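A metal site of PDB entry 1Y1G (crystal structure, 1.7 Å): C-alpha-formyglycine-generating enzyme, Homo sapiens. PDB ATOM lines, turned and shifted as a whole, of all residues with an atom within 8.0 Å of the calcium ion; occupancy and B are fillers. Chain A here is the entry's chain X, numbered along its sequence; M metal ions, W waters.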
ATOM      1  N   HIS A 184     -22.205  15.896   3.782  1.00  0.00           N
ATOM      2  CA  HIS A 184     -21.821  14.665   3.144  1.00  0.00           C
ATOM      3  C   HIS A 184     -22.676  13.536   3.702  1.00  0.00           C
ATOM      4  O   HIS A 184     -22.807  13.413   4.931  1.00  0.00           O
ATOM      5  CB  HIS A 184     -20.328  14.402   3.344  1.00  0.00           C
ATOM      6  CG  HIS A 184     -19.464  15.232   2.446  1.00  0.00           C
ATOM      7  ND1 HIS A 184     -19.338  14.985   1.097  1.00  0.00           N
ATOM      8  CD2 HIS A 184     -18.735  16.348   2.691  1.00  0.00           C
ATOM      9  CE1 HIS A 184     -18.546  15.900   0.556  1.00  0.00           C
ATOM     10  NE2 HIS A 184     -18.170  16.738   1.503  1.00  0.00           N
ATOM     11  N   ALA A 186     -22.335  10.161   2.346  1.00  0.00           N
ATOM     12  CA  ALA A 186     -21.672   8.897   1.991  1.00  0.00           C
ATOM     13  C   ALA A 186     -20.202   9.140   1.783  1.00  0.00           C
ATOM     14  O   ALA A 186     -19.754  10.265   1.507  1.00  0.00           O
ATOM     15  CB  ALA A 186     -22.273   8.303   0.735  1.00  0.00           C
ATOM     16  N   ASN A 187     -19.436   8.070   1.955  1.00  0.00           N
ATOM     17  CA  ASN A 187     -17.999   8.107   1.782  1.00  0.00           C
ATOM     18  C   ASN A 187     -17.628   7.701   0.349  1.00  0.00           C
ATOM     19  O   ASN A 187     -17.566   6.516   0.034  1.00  0.00           O
ATOM     20  CB  ASN A 187     -17.327   7.198   2.797  1.00  0.00           C
ATOM     21  CG  ASN A 187     -15.815   7.169   2.658  1.00  0.00           C
ATOM     22  OD1 ASN A 187     -15.211   8.098   2.084  1.00  0.00           O
ATOM     23  ND2 ASN A 187     -15.189   6.112   3.198  1.00  0.00           N
ATOM     24  N   ILE A 188     -17.378   8.691  -0.497  1.00  0.00           N
ATOM     25  CA  ILE A 188     -16.893   8.476  -1.866  1.00  0.00           C
ATOM     26  C   ILE A 188     -15.607   9.308  -2.080  1.00  0.00           C
ATOM     27  O   ILE A 188     -14.978   9.694  -1.105  1.00  0.00           O
ATOM     28  CB  ILE A 188     -18.011   8.783  -2.895  1.00  0.00           C
ATOM     29  CG1 ILE A 188     -18.472  10.240  -2.812  1.00  0.00           C
ATOM     30  CG2 ILE A 188     -19.174   7.830  -2.674  1.00  0.00           C
ATOM     31  CD1 ILE A 188     -19.365  10.666  -3.965  1.00  0.00           C
ATOM     32  N   TRP A 189     -15.229   9.587  -3.317  1.00  0.00           N
ATOM     33  CA  TRP A 189     -14.000  10.312  -3.587  1.00  0.00           C
ATOM     34  C   TRP A 189     -14.260  11.797  -3.788  1.00  0.00           C
ATOM     35  O   TRP A 189     -15.211  12.147  -4.487  1.00  0.00           O
ATOM     36  CB  TRP A 189     -13.363   9.738  -4.833  1.00  0.00           C
ATOM     37  CG  TRP A 189     -12.012  10.249  -5.215  1.00  0.00           C
ATOM     38  CD1 TRP A 189     -11.712  11.457  -5.816  1.00  0.00           C
ATOM     39  CD2 TRP A 189     -10.794   9.553  -5.076  1.00  0.00           C
ATOM     40  NE1 TRP A 189     -10.369  11.544  -6.031  1.00  0.00           N
ATOM     41  CE2 TRP A 189      -9.772  10.377  -5.608  1.00  0.00           C
ATOM     42  CE3 TRP A 189     -10.441   8.300  -4.561  1.00  0.00           C
ATOM     43  CZ2 TRP A 189      -8.434   9.984  -5.618  1.00  0.00           C
ATOM     44  CZ3 TRP A 189      -9.125   7.911  -4.591  1.00  0.00           C
ATOM     45  CH2 TRP A 189      -8.135   8.739  -5.133  1.00  0.00           C
ATOM     46  N   GLN A 190     -13.437  12.668  -3.209  1.00  0.00           N
ATOM     47  CA  GLN A 190     -13.414  14.066  -3.656  1.00  0.00           C
ATOM     48  C   GLN A 190     -12.025  14.367  -4.158  1.00  0.00           C
ATOM     49  O   GLN A 190     -11.039  13.887  -3.598  1.00  0.00           O
ATOM     50  CB  GLN A 190     -13.783  15.042  -2.548  1.00  0.00           C
ATOM     51  CG  GLN A 190     -15.206  14.878  -2.039  1.00  0.00           C
ATOM     52  CD  GLN A 190     -15.285  13.809  -0.970  1.00  0.00           C
ATOM     53  OE1 GLN A 190     -14.398  13.720  -0.096  1.00  0.00           O
ATOM     54  NE2 GLN A 190     -16.368  12.997  -1.011  1.00  0.00           N
ATOM     55  N   ASN A 197      -7.042  12.437  -3.538  1.00  0.00           N
ATOM     56  CA  ASN A 197      -8.266  12.347  -2.765  1.00  0.00           C
ATOM     57  C   ASN A 197      -8.153  13.359  -1.643  1.00  0.00           C
ATOM     58  O   ASN A 197      -7.297  13.226  -0.752  1.00  0.00           O
ATOM     59  CB  ASN A 197      -8.431  10.936  -2.188  1.00  0.00           C
ATOM     60  CG  ASN A 197      -9.764  10.736  -1.498  1.00  0.00           C
ATOM     61  OD1 ASN A 197     -10.352  11.680  -1.011  1.00  0.00           O
ATOM     62  ND2 ASN A 197     -10.239   9.499  -1.470  1.00  0.00           N
ATOM     63  N   THR A 198      -8.967  14.404  -1.679  1.00  0.00           N
ATOM     64  CA  THR A 198      -8.843  15.476  -0.695  1.00  0.00           C
ATOM     65  C   THR A 198      -9.324  15.093   0.709  1.00  0.00           C
ATOM     66  O   THR A 198      -8.997  15.764   1.707  1.00  0.00           O
ATOM     67  CB  THR A 198      -9.644  16.708  -1.126  1.00  0.00           C
ATOM     68  OG1 THR A 198     -11.024  16.350  -1.091  1.00  0.00           O
ATOM     69  CG2 THR A 198      -9.250  17.189  -2.507  1.00  0.00           C
ATOM     70  N   GLY A 199     -10.108  14.024   0.814  1.00  0.00           N
ATOM     71  CA  GLY A 199     -10.643  13.619   2.103  1.00  0.00           C
ATOM     72  C   GLY A 199     -11.628  14.641   2.642  1.00  0.00           C
ATOM     73  O   GLY A 199     -11.847  14.724   3.851  1.00  0.00           O
ATOM     74  N   GLU A 200     -12.273  15.373   1.745  1.00  0.00           N
ATOM     75  CA  GLU A 200     -13.281  16.356   2.148  1.00  0.00           C
ATOM     76  C   GLU A 200     -14.400  15.752   3.013  1.00  0.00           C
ATOM     77  O   GLU A 200     -14.854  16.404   4.000  1.00  0.00           O
ATOM     78  CB  GLU A 200     -13.865  17.010   0.885  1.00  0.00           C
ATOM     79  CG  GLU A 200     -14.884  18.070   1.159  1.00  0.00           C
ATOM     80  CD  GLU A 200     -15.610  18.484  -0.111  1.00  0.00           C
ATOM     81  OE1 GLU A 200     -14.998  18.462  -1.205  1.00  0.00           O
ATOM     82  OE2 GLU A 200     -16.809  18.823   0.020  1.00  0.00           O
ATOM     83  N   ASP A 201     -14.839  14.528   2.696  1.00  0.00           N
ATOM     84  CA  ASP A 201     -15.947  13.922   3.420  1.00  0.00           C
ATOM     85  C   ASP A 201     -15.519  13.319   4.765  1.00  0.00           C
ATOM     86  O   ASP A 201     -16.350  12.752   5.482  1.00  0.00           O
ATOM     87  CB  ASP A 201     -16.693  12.904   2.561  1.00  0.00           C
ATOM     88  CG  ASP A 201     -15.845  11.729   2.156  1.00  0.00           C
ATOM     89  OD1 ASP A 201     -14.805  11.492   2.808  1.00  0.00           O
ATOM     90  OD2 ASP A 201     -16.209  11.043   1.182  1.00  0.00           O
ATOM     91  N   GLY A 202     -14.224  13.421   5.085  1.00  0.00           N
ATOM     92  CA  GLY A 202     -13.703  12.962   6.370  1.00  0.00           C
ATOM     93  C   GLY A 202     -12.884  11.686   6.331  1.00  0.00           C
ATOM     94  O   GLY A 202     -12.293  11.303   7.342  1.00  0.00           O
ATOM     95  N   PHE A 203     -12.857  11.021   5.174  1.00  0.00           N
ATOM     96  CA  PHE A 203     -12.213   9.713   5.026  1.00  0.00           C
ATOM     97  C   PHE A 203     -11.627   9.556   3.646  1.00  0.00           C
ATOM     98  O   PHE A 203     -12.360   9.650   2.663  1.00  0.00           O
ATOM     99  CB  PHE A 203     -13.246   8.613   5.277  1.00  0.00           C
ATOM    100  CG  PHE A 203     -13.901   8.745   6.623  1.00  0.00           C
ATOM    101  CD1 PHE A 203     -13.287   8.213   7.741  1.00  0.00           C
ATOM    102  CD2 PHE A 203     -15.091   9.443   6.764  1.00  0.00           C
ATOM    103  CE1 PHE A 203     -13.878   8.347   8.993  1.00  0.00           C
ATOM    104  CE2 PHE A 203     -15.671   9.580   8.026  1.00  0.00           C
ATOM    105  CZ  PHE A 203     -15.046   9.039   9.133  1.00  0.00           C
ATOM    106  N   GLN A 204     -10.329   9.311   3.561  1.00  0.00           N
ATOM    107  CA  GLN A 204      -9.699   8.997   2.276  1.00  0.00           C
ATOM    108  C   GLN A 204      -9.929   7.540   1.914  1.00  0.00           C
ATOM    109  O   GLN A 204     -10.289   7.248   0.785  1.00  0.00           O
ATOM    110  CB  GLN A 204      -8.213   9.299   2.313  1.00  0.00           C
ATOM    111  CG  GLN A 204      -7.993  10.804   2.358  1.00  0.00           C
ATOM    112  CD  GLN A 204      -6.582  11.190   2.560  1.00  0.00           C
ATOM    113  OE1 GLN A 204      -5.937  10.708   3.500  1.00  0.00           O
ATOM    114  NE2 GLN A 204      -6.097  12.135   1.758  1.00  0.00           N
ATOM    115  N   GLY A 205      -9.689   6.639   2.868  1.00  0.00           N
ATOM    116  CA  GLY A 205     -10.007   5.236   2.686  1.00  0.00           C
ATOM    117  C   GLY A 205     -11.384   4.955   3.266  1.00  0.00           C
ATOM    118  O   GLY A 205     -12.278   5.770   3.117  1.00  0.00           O
ATOM    119  N   THR A 206     -11.539   3.809   3.913  1.00  0.00           N
ATOM    120  CA  THR A 206     -12.816   3.487   4.513  1.00  0.00           C
ATOM    121  C   THR A 206     -13.123   4.324   5.755  1.00  0.00           C
ATOM    122  O   THR A 206     -12.223   4.995   6.343  1.00  0.00           O
ATOM    123  CB  THR A 206     -12.886   1.982   4.904  1.00  0.00           C
ATOM    124  OG1 THR A 206     -11.801   1.695   5.780  1.00  0.00           O
ATOM    125  CG2 THR A 206     -12.803   1.084   3.659  1.00  0.00           C
ATOM    126  N   ALA A 207     -14.391   4.325   6.107  1.00  0.00           N
ATOM    127  CA  ALA A 207     -14.893   4.931   7.323  1.00  0.00           C
ATOM    128  C   ALA A 207     -15.454   3.818   8.218  1.00  0.00           C
ATOM    129  O   ALA A 207     -15.800   2.745   7.718  1.00  0.00           O
ATOM    130  CB  ALA A 207     -16.013   5.933   7.014  1.00  0.00           C
ATOM    131  N   PHE A 212     -21.753   8.303   8.839  1.00  0.00           N
ATOM    132  CA  PHE A 212     -22.726   8.935   7.939  1.00  0.00           C
ATOM    133  C   PHE A 212     -24.179   8.673   8.339  1.00  0.00           C
ATOM    134  O   PHE A 212     -24.469   7.786   9.166  1.00  0.00           O
ATOM    135  CB  PHE A 212     -22.400   8.659   6.463  1.00  0.00           C
ATOM    136  CG  PHE A 212     -21.048   9.207   6.046  1.00  0.00           C
ATOM    137  CD1 PHE A 212     -20.894  10.581   5.827  1.00  0.00           C
ATOM    138  CD2 PHE A 212     -19.955   8.398   5.993  1.00  0.00           C
ATOM    139  CE1 PHE A 212     -19.662  11.096   5.500  1.00  0.00           C
ATOM    140  CE2 PHE A 212     -18.703   8.905   5.656  1.00  0.00           C
ATOM    141  CZ  PHE A 212     -18.567  10.266   5.439  1.00  0.00           C
ATOM    142  N   ASN A 225     -18.338   3.823   0.831  1.00  0.00           N
ATOM    143  CA  ASN A 225     -17.534   3.075   1.792  1.00  0.00           C
ATOM    144  C   ASN A 225     -17.000   1.799   1.152  1.00  0.00           C
ATOM    145  O   ASN A 225     -16.065   1.906   0.350  1.00  0.00           O
ATOM    146  CB  ASN A 225     -18.245   2.880   3.136  1.00  0.00           C
ATOM    147  CG  ASN A 225     -17.276   2.971   4.319  1.00  0.00           C
ATOM    148  OD1 ASN A 225     -16.312   3.719   4.251  1.00  0.00           O
ATOM    149  ND2 ASN A 225     -17.543   2.225   5.391  1.00  0.00           N
ATOM    150  N   SER A 261     -18.173   2.749  -3.601  1.00  0.00           N
ATOM    151  CA  SER A 261     -17.177   2.749  -2.551  1.00  0.00           C
ATOM    152  C   SER A 261     -16.514   4.103  -2.359  1.00  0.00           C
ATOM    153  O   SER A 261     -16.829   5.056  -3.073  1.00  0.00           O
ATOM    154  CB  SER A 261     -16.103   1.717  -2.850  1.00  0.00           C
ATOM    155  OG  SER A 261     -15.234   2.177  -3.879  1.00  0.00           O
ATOM    156  N   TYR A 262     -15.587   4.162  -1.412  1.00  0.00           N
ATOM    157  CA  TYR A 262     -14.762   5.366  -1.172  1.00  0.00           C
ATOM    158  C   TYR A 262     -13.944   5.820  -2.369  1.00  0.00           C
ATOM    159  O   TYR A 262     -13.404   6.929  -2.365  1.00  0.00           O
ATOM    160  CB  TYR A 262     -13.837   5.122   0.010  1.00  0.00           C
ATOM    161  CG  TYR A 262     -12.765   4.078  -0.198  1.00  0.00           C
ATOM    162  CD1 TYR A 262     -12.923   2.760   0.267  1.00  0.00           C
ATOM    163  CD2 TYR A 262     -11.562   4.419  -0.786  1.00  0.00           C
ATOM    164  CE1 TYR A 262     -11.915   1.812   0.112  1.00  0.00           C
ATOM    165  CE2 TYR A 262     -10.545   3.484  -0.933  1.00  0.00           C
ATOM    166  CZ  TYR A 262     -10.719   2.190  -0.500  1.00  0.00           C
ATOM    167  OH  TYR A 262      -9.688   1.288  -0.651  1.00  0.00           O
ATOM    168  N   MET A 263     -13.856   4.977  -3.388  1.00  0.00           N
ATOM    169  CA  MET A 263     -13.111   5.312  -4.618  1.00  0.00           C
ATOM    170  C   MET A 263     -13.911   5.986  -5.712  1.00  0.00           C
ATOM    171  O   MET A 263     -13.328   6.534  -6.677  1.00  0.00           O
ATOM    172  CB  MET A 263     -12.572   4.033  -5.198  1.00  0.00           C
ATOM    173  CG  MET A 263     -11.367   3.579  -4.470  1.00  0.00           C
ATOM    174  SD  MET A 263     -10.783   2.015  -5.111  1.00  0.00           S
ATOM    175  CE  MET A 263     -10.284   2.424  -6.791  1.00  0.00           C
ATOM    176  N   OCS A 264     -15.223   5.965  -5.607  1.00  0.00           N
ATOM    177  CA  OCS A 264     -16.033   6.463  -6.711  1.00  0.00           C
ATOM    178  CB  OCS A 264     -17.432   5.932  -6.646  1.00  0.00           C
ATOM    179  SG  OCS A 264     -17.559   4.178  -7.001  1.00  0.00           S
ATOM    180  C   OCS A 264     -16.100   7.982  -6.815  1.00  0.00           C
ATOM    181  O   OCS A 264     -16.175   8.682  -5.821  1.00  0.00           O
ATOM    182  OD1 OCS A 264     -18.949   3.970  -7.184  1.00  0.00           O
ATOM    183  OD2 OCS A 264     -16.820   3.850  -8.218  1.00  0.00           O
ATOM    184  OD3 OCS A 264     -17.012   3.436  -5.918  1.00  0.00           O
HETATM  185 CA    CA M   1     -14.083   9.834   1.093  1.00  0.00          CA
HETATM  186  O   HOH W   1     -12.797  11.618   0.291  1.00  0.00           O
HETATM  187  O   HOH W   2     -12.615   8.337  -0.161  1.00  0.00           O
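The backbone carbonyl oxygen (O) of Gly 205 sits at hydrogen-bond distance from the side-chain amide nitrogen (ND2) of Asn 187, at 2.9 Å. The side-chain amide oxygen (OE1) of Gln 190 is in hydrogen-bond range of the backbone NH (N) of Asp 201 (2.9 Å). The side-chain amide oxygen of Asn 225 lies within hydrogen-bond range of the side-chain amide nitrogen of Asn 187 (2.8 Å). The backbone NH (N) of Tyr 262 lies close to the backbone carbonyl oxygen (O) of Asn 187.
Along chain A the residues within 4 Å of the calcium ion span positions 187 to 203. The nearest printed residue that does not touch the calcium ion is Gln 190 (4.1 Å).
The calcium ion is bound by OD1 of Asn 187. The backbone carbonyl oxygen (O) of Phe 203 binds the calcium ion (2.3 Å). Water W1 binds the calcium ion, at 2.3 Å. O of Ile 188 is bound to the calcium ion (2.4 Å). Water W2 is bound to the calcium ion (2.4 Å). The side-chain carboxylate (OD2) of Asp 201 binds the calcium ion (2.4 Å). The calcium ion is bound by the side-chain carboxylate (OD1) of Asp 201 (2.5 Å). The calcium ion has seven donor atoms within binding distance.
Water W1 bridges OE1 of Gln 190 and OD1 of Asn 197. Water W2 lies within hydrogen-bond range of the backbone carbonyl oxygen (O) of Tyr 262 (2.7 Å), the backbone carbonyl oxygen (O) of Gln 204 (2.7 Å) and the side-chain amide nitrogen (ND2) of Asn 197 (3.0 Å).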
